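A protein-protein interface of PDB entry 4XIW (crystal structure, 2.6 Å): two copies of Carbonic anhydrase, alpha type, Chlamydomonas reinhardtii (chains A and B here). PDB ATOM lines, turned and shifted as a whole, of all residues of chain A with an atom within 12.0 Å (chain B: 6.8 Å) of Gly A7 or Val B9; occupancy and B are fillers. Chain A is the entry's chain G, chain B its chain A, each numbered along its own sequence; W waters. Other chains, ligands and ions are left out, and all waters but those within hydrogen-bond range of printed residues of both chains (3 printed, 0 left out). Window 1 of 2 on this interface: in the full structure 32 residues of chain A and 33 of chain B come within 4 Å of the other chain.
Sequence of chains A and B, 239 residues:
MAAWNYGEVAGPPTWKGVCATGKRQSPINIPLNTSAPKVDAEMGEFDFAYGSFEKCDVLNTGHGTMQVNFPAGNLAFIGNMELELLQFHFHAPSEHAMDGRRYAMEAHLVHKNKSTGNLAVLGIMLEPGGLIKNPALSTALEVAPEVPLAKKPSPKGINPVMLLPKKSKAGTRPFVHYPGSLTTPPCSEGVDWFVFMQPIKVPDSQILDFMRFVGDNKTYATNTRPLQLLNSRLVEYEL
The backbone NH (N) of Gly A11 sits at hydrogen-bond distance from the backbone carbonyl oxygen (O) of Tyr B6 (2.8 Å). The side-chain hydroxyl (OH) of Tyr B6 is in hydrogen-bond range of the backbone carbonyl oxygen (O) of Asn A223, at 3.4 Å. The backbone NH of Ala B10 sits at hydrogen-bond distance from the backbone carbonyl oxygen of Glu A8 (2.7 Å). The backbone carbonyl oxygen (O) of Glu B8 lies within hydrogen-bond range of the backbone NH (N) of Ala A10 (2.7 Å). The side-chain hydroxyl (OH) of Tyr A6 is in hydrogen-bond range of the backbone carbonyl oxygen (O) of Asn B223 (3.3 Å). The backbone carbonyl oxygen (O) of Tyr A6 is in hydrogen-bond range of the backbone NH (N) of Gly B11 (2.8 Å). N of Ala B10 lies within hydrogen-bond range of O of Tyr A6, at 3.5 Å. The backbone NH (N) of Ala A10 sits at hydrogen-bond distance from the backbone carbonyl oxygen (O) of Tyr B6, at 3.3 Å.
Water W1 lies within hydrogen-bond range of the side-chain hydroxyl of Tyr B6 (2.8 Å) and the backbone NH of Arg A225 (3.4 Å). Water W2 bridges OH of Tyr A6 (2.8 Å) and ND2 of Asn B223 (3.0 Å). Water W3 lies within hydrogen-bond range of the backbone NH (N) of Asn A5 and the backbone carbonyl oxygen (O) of Gly B11.
The backbone carbonyl oxygen (O) of Pro A93 lies within hydrogen-bond range of the side-chain hydroxyl (OG1) of Thr A224, 2.4 Å away. OG1 of Thr A14 sits at hydrogen-bond distance from O of Gly A11, at 2.8 Å. OD1 of Asn A5 sits at hydrogen-bond distance from N of Gly A7 (3.2 Å). OD1 of Asn A223 lies within hydrogen-bond range of N of Ala A92 (2.9 Å). O of Ala A92 lies within hydrogen-bond range of OG1 of Thr A224.
CE1 of Tyr A6 touches N of Thr B224, at 3.6 Å. O of Gly A7 touches CG1 of Val B9, at 3.6 Å. O of Glu A8 touches O of Glu B8, 3.9 Å away. Val B9 touches Glu A8. Val A9 touches Tyr B6. Val A9 touches Gly B7. Val A9 touches Glu B8 (CA to O, 3.4 Å). CB of Ala A10 touches CB of Ala B10 (3.8 Å). Tyr B6 touches Pro A12. Tyr B6 touches Thr A224.
Tyr A6 touches Asn B223, and with the chains exchanged Asn A223 touches Tyr B6. Gly A7 touches Val B9, and with the chains exchanged Val A9 touches Gly B7. Val B9 touches its own counterpart, Val A9. Ala A10 touches its own counterpart, Ala B10. 14 positions are printed for both chains.
Of the printed residues of chain B, Asn A5 touches Gly B11. Of the printed residues of chain B, Tyr A6 touches Val B9 (3.1 Å), Ala B10 (3.5 Å), Gly B11 (2.8 Å), Pro B12 (3.3 Å), Asn B223 (3.3 Å), Thr B224 (3.6 Å) and Arg B225 (3.96 Å). Of chain B, only Val B9 comes within 4 Å of Gly A7. Of the printed residues of chain B, Gly A11 touches Tyr B6. Gly A215 touches none of the printed residues of chain B. Arg A225 touches none of the printed residues of chain B. Glu B8 touches just these residues of chain A: Glu A8 (3.9 Å), Val A9 (3.4 Å) and Ala A10 (2.7 Å). Val B9 touches four residues of chain A. Gly B11 touches two residues of chain A. Pro B12 touches just one residue of chain A: Tyr A6. No residue of chain A comes within 4 Å of Thr B222. The nearest residue of chain A that does not touch Val B9 is Ala A10 (4.5 Å).
Of the 26 printed residues of chain A, 10 touch a printed residue of chain B. Among the printed residues, 23 pairs touch across the chains. Among the printed residues, no Asp or Glu carboxylate lies within 4 Å of a Lys or Arg side-chain nitrogen of the other chain.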
ATOM      1  N   ALA A   3     -20.754   2.557   5.974  1.00  0.00           N
ATOM      2  CA  ALA A   3     -20.587   3.855   6.680  1.00  0.00           C
ATOM      3  C   ALA A   3     -20.406   3.667   8.186  1.00  0.00           C
ATOM      4  O   ALA A   3     -21.272   3.087   8.841  1.00  0.00           O
ATOM      5  CB  ALA A   3     -21.782   4.748   6.419  1.00  0.00           C
ATOM      6  N   TRP A   4     -19.294   4.147   8.742  1.00  0.00           N
ATOM      7  CA  TRP A   4     -18.962   3.811  10.132  1.00  0.00           C
ATOM      8  C   TRP A   4     -18.107   4.864  10.825  1.00  0.00           C
ATOM      9  O   TRP A   4     -17.395   5.655  10.185  1.00  0.00           O
ATOM     10  CB  TRP A   4     -18.246   2.450  10.202  1.00  0.00           C
ATOM     11  CG  TRP A   4     -16.825   2.496   9.642  1.00  0.00           C
ATOM     12  CD1 TRP A   4     -16.452   2.301   8.350  1.00  0.00           C
ATOM     13  CD2 TRP A   4     -15.611   2.765  10.369  1.00  0.00           C
ATOM     14  NE1 TRP A   4     -15.094   2.444   8.218  1.00  0.00           N
ATOM     15  CE2 TRP A   4     -14.555   2.729   9.442  1.00  0.00           C
ATOM     16  CE3 TRP A   4     -15.325   3.050  11.706  1.00  0.00           C
ATOM     17  CZ2 TRP A   4     -13.236   2.954   9.807  1.00  0.00           C
ATOM     18  CZ3 TRP A   4     -14.024   3.276  12.068  1.00  0.00           C
ATOM     19  CH2 TRP A   4     -12.987   3.225  11.123  1.00  0.00           C
ATOM     20  N   ASN A   5     -18.177   4.852  12.149  1.00  0.00           N
ATOM     21  CA  ASN A   5     -17.442   5.795  12.970  1.00  0.00           C
ATOM     22  C   ASN A   5     -17.134   5.150  14.302  1.00  0.00           C
ATOM     23  O   ASN A   5     -17.601   4.026  14.599  1.00  0.00           O
ATOM     24  CB  ASN A   5     -18.307   7.009  13.223  1.00  0.00           C
ATOM     25  CG  ASN A   5     -19.733   6.624  13.645  1.00  0.00           C
ATOM     26  OD1 ASN A   5     -20.032   6.427  14.847  1.00  0.00           O
ATOM     27  ND2 ASN A   5     -20.618   6.482  12.645  1.00  0.00           N
ATOM     28  N   TYR A   6     -16.355   5.855  15.117  1.00  0.00           N
ATOM     29  CA  TYR A   6     -16.141   5.413  16.493  1.00  0.00           C
ATOM     30  C   TYR A   6     -17.273   5.981  17.299  1.00  0.00           C
ATOM     31  O   TYR A   6     -17.822   5.337  18.200  1.00  0.00           O
ATOM     32  CB  TYR A   6     -14.787   5.876  17.015  1.00  0.00           C
ATOM     33  CG  TYR A   6     -13.654   5.125  16.350  1.00  0.00           C
ATOM     34  CD1 TYR A   6     -13.289   3.853  16.777  1.00  0.00           C
ATOM     35  CD2 TYR A   6     -12.996   5.659  15.275  1.00  0.00           C
ATOM     36  CE1 TYR A   6     -12.278   3.132  16.143  1.00  0.00           C
ATOM     37  CE2 TYR A   6     -11.962   4.946  14.631  1.00  0.00           C
ATOM     38  CZ  TYR A   6     -11.611   3.691  15.073  1.00  0.00           C
ATOM     39  OH  TYR A   6     -10.593   3.022  14.461  1.00  0.00           O
ATOM     40  N   GLY A   7     -17.656   7.187  16.914  1.00  0.00           N
ATOM     41  CA  GLY A   7     -18.789   7.847  17.512  1.00  0.00           C
ATOM     42  C   GLY A   7     -18.465   8.417  18.881  1.00  0.00           C
ATOM     43  O   GLY A   7     -17.291   8.537  19.261  1.00  0.00           O
ATOM     44  N   GLU A   8     -19.490   8.723  19.649  1.00  0.00           N
ATOM     45  CA  GLU A   8     -19.268   9.336  20.920  1.00  0.00           C
ATOM     46  C   GLU A   8     -19.600   8.376  21.987  1.00  0.00           C
ATOM     47  O   GLU A   8     -19.978   7.282  21.695  1.00  0.00           O
ATOM     48  CB  GLU A   8     -20.105  10.575  21.050  1.00  0.00           C
ATOM     49  CG  GLU A   8     -19.417  11.802  20.535  1.00  0.00           C
ATOM     50  CD  GLU A   8     -19.488  11.930  19.032  1.00  0.00           C
ATOM     51  OE1 GLU A   8     -19.592  10.925  18.348  1.00  0.00           O
ATOM     52  OE2 GLU A   8     -19.439  13.037  18.513  1.00  0.00           O
ATOM     53  N   VAL A   9     -19.422   8.770  23.226  1.00  0.00           N
ATOM     54  CA  VAL A   9     -19.733   7.867  24.318  1.00  0.00           C
ATOM     55  C   VAL A   9     -21.238   7.585  24.298  1.00  0.00           C
ATOM     56  O   VAL A   9     -22.042   8.460  23.966  1.00  0.00           O
ATOM     57  CB  VAL A   9     -19.230   8.399  25.680  1.00  0.00           C
ATOM     58  CG1 VAL A   9     -17.692   8.453  25.648  1.00  0.00           C
ATOM     59  CG2 VAL A   9     -19.887   9.770  26.041  1.00  0.00           C
ATOM     60  N   ALA A  10     -21.595   6.341  24.605  1.00  0.00           N
ATOM     61  CA  ALA A  10     -22.937   5.820  24.352  1.00  0.00           C
ATOM     62  C   ALA A  10     -23.984   6.248  25.365  1.00  0.00           C
ATOM     63  O   ALA A  10     -25.170   6.291  25.039  1.00  0.00           O
ATOM     64  CB  ALA A  10     -22.890   4.303  24.291  1.00  0.00           C
ATOM     65  N   GLY A  11     -23.539   6.558  26.580  1.00  0.00           N
ATOM     66  CA  GLY A  11     -24.424   6.803  27.703  1.00  0.00           C
ATOM     67  C   GLY A  11     -25.301   8.052  27.674  1.00  0.00           C
ATOM     68  O   GLY A  11     -26.525   7.964  27.859  1.00  0.00           O
ATOM     69  N   PRO A  12     -24.689   9.230  27.474  1.00  0.00           N
ATOM     70  CA  PRO A  12     -25.439  10.494  27.610  1.00  0.00           C
ATOM     71  C   PRO A  12     -26.735  10.619  26.785  1.00  0.00           C
ATOM     72  O   PRO A  12     -27.706  11.158  27.319  1.00  0.00           O
ATOM     73  CB  PRO A  12     -24.410  11.564  27.215  1.00  0.00           C
ATOM     74  CG  PRO A  12     -23.101  10.954  27.595  1.00  0.00           C
ATOM     75  CD  PRO A  12     -23.249   9.467  27.278  1.00  0.00           C
ATOM     76  N   PRO A  13     -26.774  10.139  25.531  1.00  0.00           N
ATOM     77  CA  PRO A  13     -28.054  10.277  24.813  1.00  0.00           C
ATOM     78  C   PRO A  13     -29.175   9.362  25.326  1.00  0.00           C
ATOM     79  O   PRO A  13     -30.265   9.362  24.763  1.00  0.00           O
ATOM     80  CB  PRO A  13     -27.690   9.911  23.372  1.00  0.00           C
ATOM     81  CG  PRO A  13     -26.436   9.091  23.485  1.00  0.00           C
ATOM     82  CD  PRO A  13     -25.699   9.632  24.665  1.00  0.00           C
ATOM     83  N   THR A  14     -28.912   8.599  26.382  1.00  0.00           N
ATOM     84  CA  THR A  14     -29.899   7.684  26.956  1.00  0.00           C
ATOM     85  C   THR A  14     -30.244   8.052  28.405  1.00  0.00           C
ATOM     86  O   THR A  14     -31.007   7.335  29.059  1.00  0.00           O
ATOM     87  CB  THR A  14     -29.381   6.219  26.943  1.00  0.00           C
ATOM     88  OG1 THR A  14     -28.518   5.994  28.072  1.00  0.00           O
ATOM     89  CG2 THR A  14     -28.638   5.913  25.634  1.00  0.00           C
ATOM     90  N   ALA A  92     -12.976  15.947  30.954  1.00  0.00           N
ATOM     91  CA  ALA A  92     -12.040  15.930  29.816  1.00  0.00           C
ATOM     92  C   ALA A  92     -12.752  15.263  28.663  1.00  0.00           C
ATOM     93  O   ALA A  92     -13.323  14.182  28.847  1.00  0.00           O
ATOM     94  CB  ALA A  92     -10.835  15.139  30.168  1.00  0.00           C
ATOM     95  N   PRO A  93     -12.787  15.914  27.481  1.00  0.00           N
ATOM     96  CA  PRO A  93     -12.386  17.301  27.248  1.00  0.00           C
ATOM     97  C   PRO A  93     -13.442  18.201  27.932  1.00  0.00           C
ATOM     98  O   PRO A  93     -14.264  17.695  28.699  1.00  0.00           O
ATOM     99  CB  PRO A  93     -12.452  17.434  25.740  1.00  0.00           C
ATOM    100  CG  PRO A  93     -13.569  16.484  25.347  1.00  0.00           C
ATOM    101  CD  PRO A  93     -13.447  15.328  26.296  1.00  0.00           C
ATOM    102  N   ARG A 102     -13.918  22.920  21.969  1.00  0.00           N
ATOM    103  CA  ARG A 102     -13.684  22.477  23.342  1.00  0.00           C
ATOM    104  C   ARG A 102     -12.208  22.500  23.765  1.00  0.00           C
ATOM    105  O   ARG A 102     -11.305  22.591  22.947  1.00  0.00           O
ATOM    106  CB  ARG A 102     -14.250  21.073  23.516  1.00  0.00           C
ATOM    107  CG  ARG A 102     -15.746  21.084  23.663  1.00  0.00           C
ATOM    108  CD  ARG A 102     -16.355  19.709  23.800  1.00  0.00           C
ATOM    109  NE  ARG A 102     -17.691  19.810  24.374  1.00  0.00           N
ATOM    110  CZ  ARG A 102     -18.552  18.806  24.478  1.00  0.00           C
ATOM    111  NH1 ARG A 102     -18.248  17.596  24.016  1.00  0.00           N
ATOM    112  NH2 ARG A 102     -19.722  19.028  25.060  1.00  0.00           N
ATOM    113  N   MET A 211      -7.168  12.045  32.293  1.00  0.00           N
ATOM    114  CA  MET A 211      -7.838  11.113  31.370  1.00  0.00           C
ATOM    115  C   MET A 211      -7.537   9.655  31.746  1.00  0.00           C
ATOM    116  O   MET A 211      -8.361   8.745  31.518  1.00  0.00           O
ATOM    117  CB  MET A 211      -7.372  11.347  29.950  1.00  0.00           C
ATOM    118  CG  MET A 211      -7.685  12.699  29.445  1.00  0.00           C
ATOM    119  SD  MET A 211      -7.041  12.934  27.787  1.00  0.00           S
ATOM    120  CE  MET A 211      -8.266  12.003  26.844  1.00  0.00           C
ATOM    121  N   VAL A 214      -9.810   8.881  34.695  1.00  0.00           N
ATOM    122  CA  VAL A 214     -11.116   8.597  34.102  1.00  0.00           C
ATOM    123  C   VAL A 214     -11.195   7.201  33.519  1.00  0.00           C
ATOM    124  O   VAL A 214     -12.243   6.585  33.527  1.00  0.00           O
ATOM    125  CB  VAL A 214     -11.450   9.607  33.004  1.00  0.00           C
ATOM    126  CG1 VAL A 214     -12.718   9.220  32.238  1.00  0.00           C
ATOM    127  CG2 VAL A 214     -11.599  11.016  33.601  1.00  0.00           C
ATOM    128  N   GLY A 215     -10.084   6.692  33.004  1.00  0.00           N
ATOM    129  CA  GLY A 215     -10.081   5.344  32.465  1.00  0.00           C
ATOM    130  C   GLY A 215      -9.739   4.274  33.488  1.00  0.00           C
ATOM    131  O   GLY A 215      -8.991   3.369  33.147  1.00  0.00           O
ATOM    132  N   THR A 219      -6.672   2.752  31.047  1.00  0.00           N
ATOM    133  CA  THR A 219      -6.778   3.271  29.682  1.00  0.00           C
ATOM    134  C   THR A 219      -6.867   4.802  29.779  1.00  0.00           C
ATOM    135  O   THR A 219      -6.605   5.389  30.836  1.00  0.00           O
ATOM    136  CB  THR A 219      -8.013   2.655  28.917  1.00  0.00           C
ATOM    137  OG1 THR A 219      -7.964   2.949  27.513  1.00  0.00           O
ATOM    138  CG2 THR A 219      -9.290   3.175  29.451  1.00  0.00           C
ATOM    139  N   TYR A 220      -7.191   5.443  28.667  1.00  0.00           N
ATOM    140  CA  TYR A 220      -7.407   6.873  28.653  1.00  0.00           C
ATOM    141  C   TYR A 220      -8.827   7.076  28.114  1.00  0.00           C
ATOM    142  O   TYR A 220      -9.224   6.428  27.122  1.00  0.00           O
ATOM    143  CB  TYR A 220      -6.352   7.568  27.809  1.00  0.00           C
ATOM    144  CG  TYR A 220      -4.955   7.460  28.374  1.00  0.00           C
ATOM    145  CD1 TYR A 220      -4.134   6.345  28.097  1.00  0.00           C
ATOM    146  CD2 TYR A 220      -4.445   8.458  29.175  1.00  0.00           C
ATOM    147  CE1 TYR A 220      -2.869   6.242  28.618  1.00  0.00           C
ATOM    148  CE2 TYR A 220      -3.180   8.362  29.686  1.00  0.00           C
ATOM    149  CZ  TYR A 220      -2.400   7.252  29.405  1.00  0.00           C
ATOM    150  OH  TYR A 220      -1.145   7.187  29.954  1.00  0.00           O
ATOM    151  N   ALA A 221      -9.591   7.924  28.812  1.00  0.00           N
ATOM    152  CA  ALA A 221     -11.011   8.121  28.532  1.00  0.00           C
ATOM    153  C   ALA A 221     -11.537   9.546  28.827  1.00  0.00           C
ATOM    154  O   ALA A 221     -10.860  10.400  29.419  1.00  0.00           O
ATOM    155  CB  ALA A 221     -11.833   7.119  29.306  1.00  0.00           C
ATOM    156  N   THR A 222     -12.769   9.772  28.393  1.00  0.00           N
ATOM    157  CA  THR A 222     -13.393  11.071  28.449  1.00  0.00           C
ATOM    158  C   THR A 222     -14.618  10.953  29.340  1.00  0.00           C
ATOM    159  O   THR A 222     -15.090   9.832  29.561  1.00  0.00           O
ATOM    160  CB  THR A 222     -13.773  11.554  27.039  1.00  0.00           C
ATOM    161  OG1 THR A 222     -14.477  10.520  26.331  1.00  0.00           O
ATOM    162  CG2 THR A 222     -12.520  11.931  26.254  1.00  0.00           C
ATOM    163  N   ASN A 223     -15.082  12.084  29.886  1.00  0.00           N
ATOM    164  CA  ASN A 223     -16.289  12.111  30.722  1.00  0.00           C
ATOM    165  C   ASN A 223     -17.046  13.413  30.530  1.00  0.00           C
ATOM    166  O   ASN A 223     -17.195  14.168  31.457  1.00  0.00           O
ATOM    167  CB  ASN A 223     -15.977  11.903  32.219  1.00  0.00           C
ATOM    168  CG  ASN A 223     -15.145  13.028  32.816  1.00  0.00           C
ATOM    169  OD1 ASN A 223     -14.371  13.656  32.105  1.00  0.00           O
ATOM    170  ND2 ASN A 223     -15.311  13.298  34.122  1.00  0.00           N
ATOM    171  N   THR A 224     -17.560  13.633  29.328  1.00  0.00           N
ATOM    172  CA  THR A 224     -18.169  14.876  28.931  1.00  0.00           C
ATOM    173  C   THR A 224     -19.527  14.622  28.302  1.00  0.00           C
ATOM    174  O   THR A 224     -19.742  13.641  27.634  1.00  0.00           O
ATOM    175  CB  THR A 224     -17.256  15.593  27.910  1.00  0.00           C
ATOM    176  OG1 THR A 224     -16.113  16.103  28.597  1.00  0.00           O
ATOM    177  CG2 THR A 224     -17.923  16.771  27.219  1.00  0.00           C
ATOM    178  N   ARG A 225     -20.452  15.542  28.510  1.00  0.00           N
ATOM    179  CA  ARG A 225     -21.747  15.462  27.869  1.00  0.00           C
ATOM    180  C   ARG A 225     -21.762  16.269  26.565  1.00  0.00           C
ATOM    181  O   ARG A 225     -21.080  17.285  26.418  1.00  0.00           O
ATOM    182  CB  ARG A 225     -22.793  16.016  28.823  1.00  0.00           C
ATOM    183  CG  ARG A 225     -24.203  15.890  28.334  1.00  0.00           C
ATOM    184  CD  ARG A 225     -25.110  16.504  29.335  1.00  0.00           C
ATOM    185  NE  ARG A 225     -26.489  16.238  28.979  1.00  0.00           N
ATOM    186  CZ  ARG A 225     -27.517  16.962  29.384  1.00  0.00           C
ATOM    187  NH1 ARG A 225     -27.327  18.000  30.179  1.00  0.00           N
ATOM    188  NH2 ARG A 225     -28.731  16.626  28.995  1.00  0.00           N
ATOM    189  N   PRO A 226     -22.552  15.828  25.602  1.00  0.00           N
ATOM    190  CA  PRO A 226     -22.642  16.669  24.408  1.00  0.00           C
ATOM    191  C   PRO A 226     -23.285  18.025  24.685  1.00  0.00           C
ATOM    192  O   PRO A 226     -23.932  18.182  25.723  1.00  0.00           O
ATOM    193  CB  PRO A 226     -23.521  15.858  23.473  1.00  0.00           C
ATOM    194  CG  PRO A 226     -23.576  14.491  24.074  1.00  0.00           C
ATOM    195  CD  PRO A 226     -23.370  14.611  25.511  1.00  0.00           C
ATOM    196  N   TYR B   6     -21.206   7.469  31.308  1.00  0.00           N
ATOM    197  CA  TYR B   6     -20.821   8.018  30.028  1.00  0.00           C
ATOM    198  C   TYR B   6     -20.685   6.894  28.975  1.00  0.00           C
ATOM    199  O   TYR B   6     -21.127   7.022  27.831  1.00  0.00           O
ATOM    200  CB  TYR B   6     -19.490   8.741  30.191  1.00  0.00           C
ATOM    201  CG  TYR B   6     -19.580   9.946  31.065  1.00  0.00           C
ATOM    202  CD1 TYR B   6     -19.998  11.164  30.540  1.00  0.00           C
ATOM    203  CD2 TYR B   6     -19.262   9.880  32.419  1.00  0.00           C
ATOM    204  CE1 TYR B   6     -20.090  12.286  31.322  1.00  0.00           C
ATOM    205  CE2 TYR B   6     -19.351  10.999  33.218  1.00  0.00           C
ATOM    206  CZ  TYR B   6     -19.770  12.211  32.663  1.00  0.00           C
ATOM    207  OH  TYR B   6     -19.890  13.369  33.445  1.00  0.00           O
ATOM    208  N   GLY B   7     -20.041   5.803  29.373  1.00  0.00           N
ATOM    209  CA  GLY B   7     -19.898   4.635  28.527  1.00  0.00           C
ATOM    210  C   GLY B   7     -18.715   4.653  27.562  1.00  0.00           C
ATOM    211  O   GLY B   7     -17.840   5.534  27.598  1.00  0.00           O
ATOM    212  N   GLU B   8     -18.690   3.636  26.707  1.00  0.00           N
ATOM    213  CA  GLU B   8     -17.739   3.575  25.609  1.00  0.00           C
ATOM    214  C   GLU B   8     -18.362   4.220  24.389  1.00  0.00           C
ATOM    215  O   GLU B   8     -19.566   4.503  24.377  1.00  0.00           O
ATOM    216  CB  GLU B   8     -17.343   2.126  25.306  1.00  0.00           C
ATOM    217  CG  GLU B   8     -16.675   1.404  26.476  1.00  0.00           C
ATOM    218  CD  GLU B   8     -15.484   2.171  27.046  1.00  0.00           C
ATOM    219  OE1 GLU B   8     -14.677   2.718  26.243  1.00  0.00           O
ATOM    220  OE2 GLU B   8     -15.373   2.237  28.300  1.00  0.00           O
ATOM    221  N   VAL B   9     -17.542   4.465  23.371  1.00  0.00           N
ATOM    222  CA  VAL B   9     -18.039   5.085  22.154  1.00  0.00           C
ATOM    223  C   VAL B   9     -19.146   4.169  21.580  1.00  0.00           C
ATOM    224  O   VAL B   9     -19.225   2.996  21.918  1.00  0.00           O
ATOM    225  CB  VAL B   9     -16.881   5.444  21.159  1.00  0.00           C
ATOM    226  CG1 VAL B   9     -15.908   6.435  21.805  1.00  0.00           C
ATOM    227  CG2 VAL B   9     -16.142   4.211  20.682  1.00  0.00           C
ATOM    228  N   ALA B  10     -20.059   4.710  20.794  1.00  0.00           N
ATOM    229  CA  ALA B  10     -21.258   3.944  20.466  1.00  0.00           C
ATOM    230  C   ALA B  10     -21.074   3.278  19.119  1.00  0.00           C
ATOM    231  O   ALA B  10     -21.862   2.409  18.739  1.00  0.00           O
ATOM    232  CB  ALA B  10     -22.544   4.849  20.511  1.00  0.00           C
ATOM    233  N   GLY B  11     -20.019   3.678  18.409  1.00  0.00           N
ATOM    234  CA  GLY B  11     -19.798   3.231  17.042  1.00  0.00           C
ATOM    235  C   GLY B  11     -19.505   1.741  16.845  1.00  0.00           C
ATOM    236  O   GLY B  11     -20.260   1.065  16.135  1.00  0.00           O
ATOM    237  N   PRO B  12     -18.407   1.235  17.455  1.00  0.00           N
ATOM    238  CA  PRO B  12     -17.888  -0.128  17.225  1.00  0.00           C
ATOM    239  C   PRO B  12     -18.833  -1.286  17.568  1.00  0.00           C
ATOM    240  O   PRO B  12     -18.796  -2.313  16.903  1.00  0.00           O
ATOM    241  CB  PRO B  12     -16.628  -0.175  18.104  1.00  0.00           C
ATOM    242  CG  PRO B  12     -16.185   1.245  18.210  1.00  0.00           C
ATOM    243  CD  PRO B  12     -17.465   2.046  18.252  1.00  0.00           C
ATOM    244  N   PRO B  13     -19.668  -1.134  18.583  1.00  0.00           N
ATOM    245  CA  PRO B  13     -20.607  -2.234  18.825  1.00  0.00           C
ATOM    246  C   PRO B  13     -21.675  -2.367  17.747  1.00  0.00           C
ATOM    247  O   PRO B  13     -22.429  -3.332  17.769  1.00  0.00           O
ATOM    248  CB  PRO B  13     -21.267  -1.849  20.149  1.00  0.00           C
ATOM    249  CG  PRO B  13     -20.295  -0.871  20.803  1.00  0.00           C
ATOM    250  CD  PRO B  13     -19.689  -0.126  19.656  1.00  0.00           C
ATOM    251  N   ALA B 221     -10.597  13.478  21.110  1.00  0.00           N
ATOM    252  CA  ALA B 221     -11.376  12.268  20.954  1.00  0.00           C
ATOM    253  C   ALA B 221     -10.434  11.078  20.927  1.00  0.00           C
ATOM    254  O   ALA B 221      -9.209  11.239  20.817  1.00  0.00           O
ATOM    255  CB  ALA B 221     -12.127  12.328  19.690  1.00  0.00           C
ATOM    256  N   THR B 222     -11.029   9.891  21.005  1.00  0.00           N
ATOM    257  CA  THR B 222     -10.318   8.652  20.782  1.00  0.00           C
ATOM    258  C   THR B 222     -10.752   7.961  19.470  1.00  0.00           C
ATOM    259  O   THR B 222     -11.773   8.320  18.888  1.00  0.00           O
ATOM    260  CB  THR B 222     -10.598   7.720  21.929  1.00  0.00           C
ATOM    261  OG1 THR B 222     -11.966   7.324  21.864  1.00  0.00           O
ATOM    262  CG2 THR B 222     -10.298   8.420  23.231  1.00  0.00           C
ATOM    263  N   ASN B 223      -9.978   6.969  19.021  1.00  0.00           N
ATOM    264  CA  ASN B 223     -10.265   6.227  17.782  1.00  0.00           C
ATOM    265  C   ASN B 223      -9.778   4.789  17.914  1.00  0.00           C
ATOM    266  O   ASN B 223      -8.987   4.283  17.087  1.00  0.00           O
ATOM    267  CB  ASN B 223      -9.609   6.882  16.559  1.00  0.00           C
ATOM    268  CG  ASN B 223      -8.106   6.781  16.589  1.00  0.00           C
ATOM    269  OD1 ASN B 223      -7.512   6.790  17.660  1.00  0.00           O
ATOM    270  ND2 ASN B 223      -7.477   6.646  15.416  1.00  0.00           N
ATOM    271  N   THR B 224     -10.283   4.131  18.956  1.00  0.00           N
ATOM    272  CA  THR B 224      -9.875   2.788  19.279  1.00  0.00           C
ATOM    273  C   THR B 224     -11.066   1.886  19.410  1.00  0.00           C
ATOM    274  O   THR B 224     -12.099   2.280  19.946  1.00  0.00           O
ATOM    275  CB  THR B 224      -9.061   2.783  20.582  1.00  0.00           C
ATOM    276  OG1 THR B 224      -7.701   3.123  20.282  1.00  0.00           O
ATOM    277  CG2 THR B 224      -9.072   1.407  21.287  1.00  0.00           C
ATOM    278  N   ARG B 225     -10.894   0.664  18.918  1.00  0.00           N
ATOM    279  CA  ARG B 225     -11.893  -0.382  18.996  1.00  0.00           C
ATOM    280  C   ARG B 225     -11.780  -1.104  20.336  1.00  0.00           C
ATOM    281  O   ARG B 225     -10.688  -1.239  20.912  1.00  0.00           O
ATOM    282  CB  ARG B 225     -11.668  -1.370  17.841  1.00  0.00           C
ATOM    283  CG  ARG B 225     -12.712  -2.483  17.785  1.00  0.00           C
ATOM    284  CD  ARG B 225     -12.391  -3.567  16.747  1.00  0.00           C
ATOM    285  NE  ARG B 225     -13.585  -4.359  16.474  1.00  0.00           N
ATOM    286  CZ  ARG B 225     -13.619  -5.505  15.812  1.00  0.00           C
ATOM    287  NH1 ARG B 225     -12.499  -6.040  15.325  1.00  0.00           N
ATOM    288  NH2 ARG B 225     -14.789  -6.122  15.643  1.00  0.00           N
ATOM    289  N   PRO B 226     -12.901  -1.582  20.861  1.00  0.00           N
ATOM    290  CA  PRO B 226     -12.707  -2.269  22.142  1.00  0.00           C
ATOM    291  C   PRO B 226     -12.071  -3.632  21.978  1.00  0.00           C
ATOM    292  O   PRO B 226     -12.295  -4.269  20.954  1.00  0.00           O
ATOM    293  CB  PRO B 226     -14.123  -2.433  22.677  1.00  0.00           C
ATOM    294  CG  PRO B 226     -15.048  -2.139  21.492  1.00  0.00           C
ATOM    295  CD  PRO B 226     -14.303  -1.185  20.641  1.00  0.00           C
HETATM  296  O   HOH W   1     -21.356  15.094  31.784  1.00  0.00           O
HETATM  297  O   HOH W   2      -9.131   5.209  13.400  1.00  0.00           O
HETATM  298  O   HOH W   3     -20.421   3.208  13.498  1.00  0.00           O
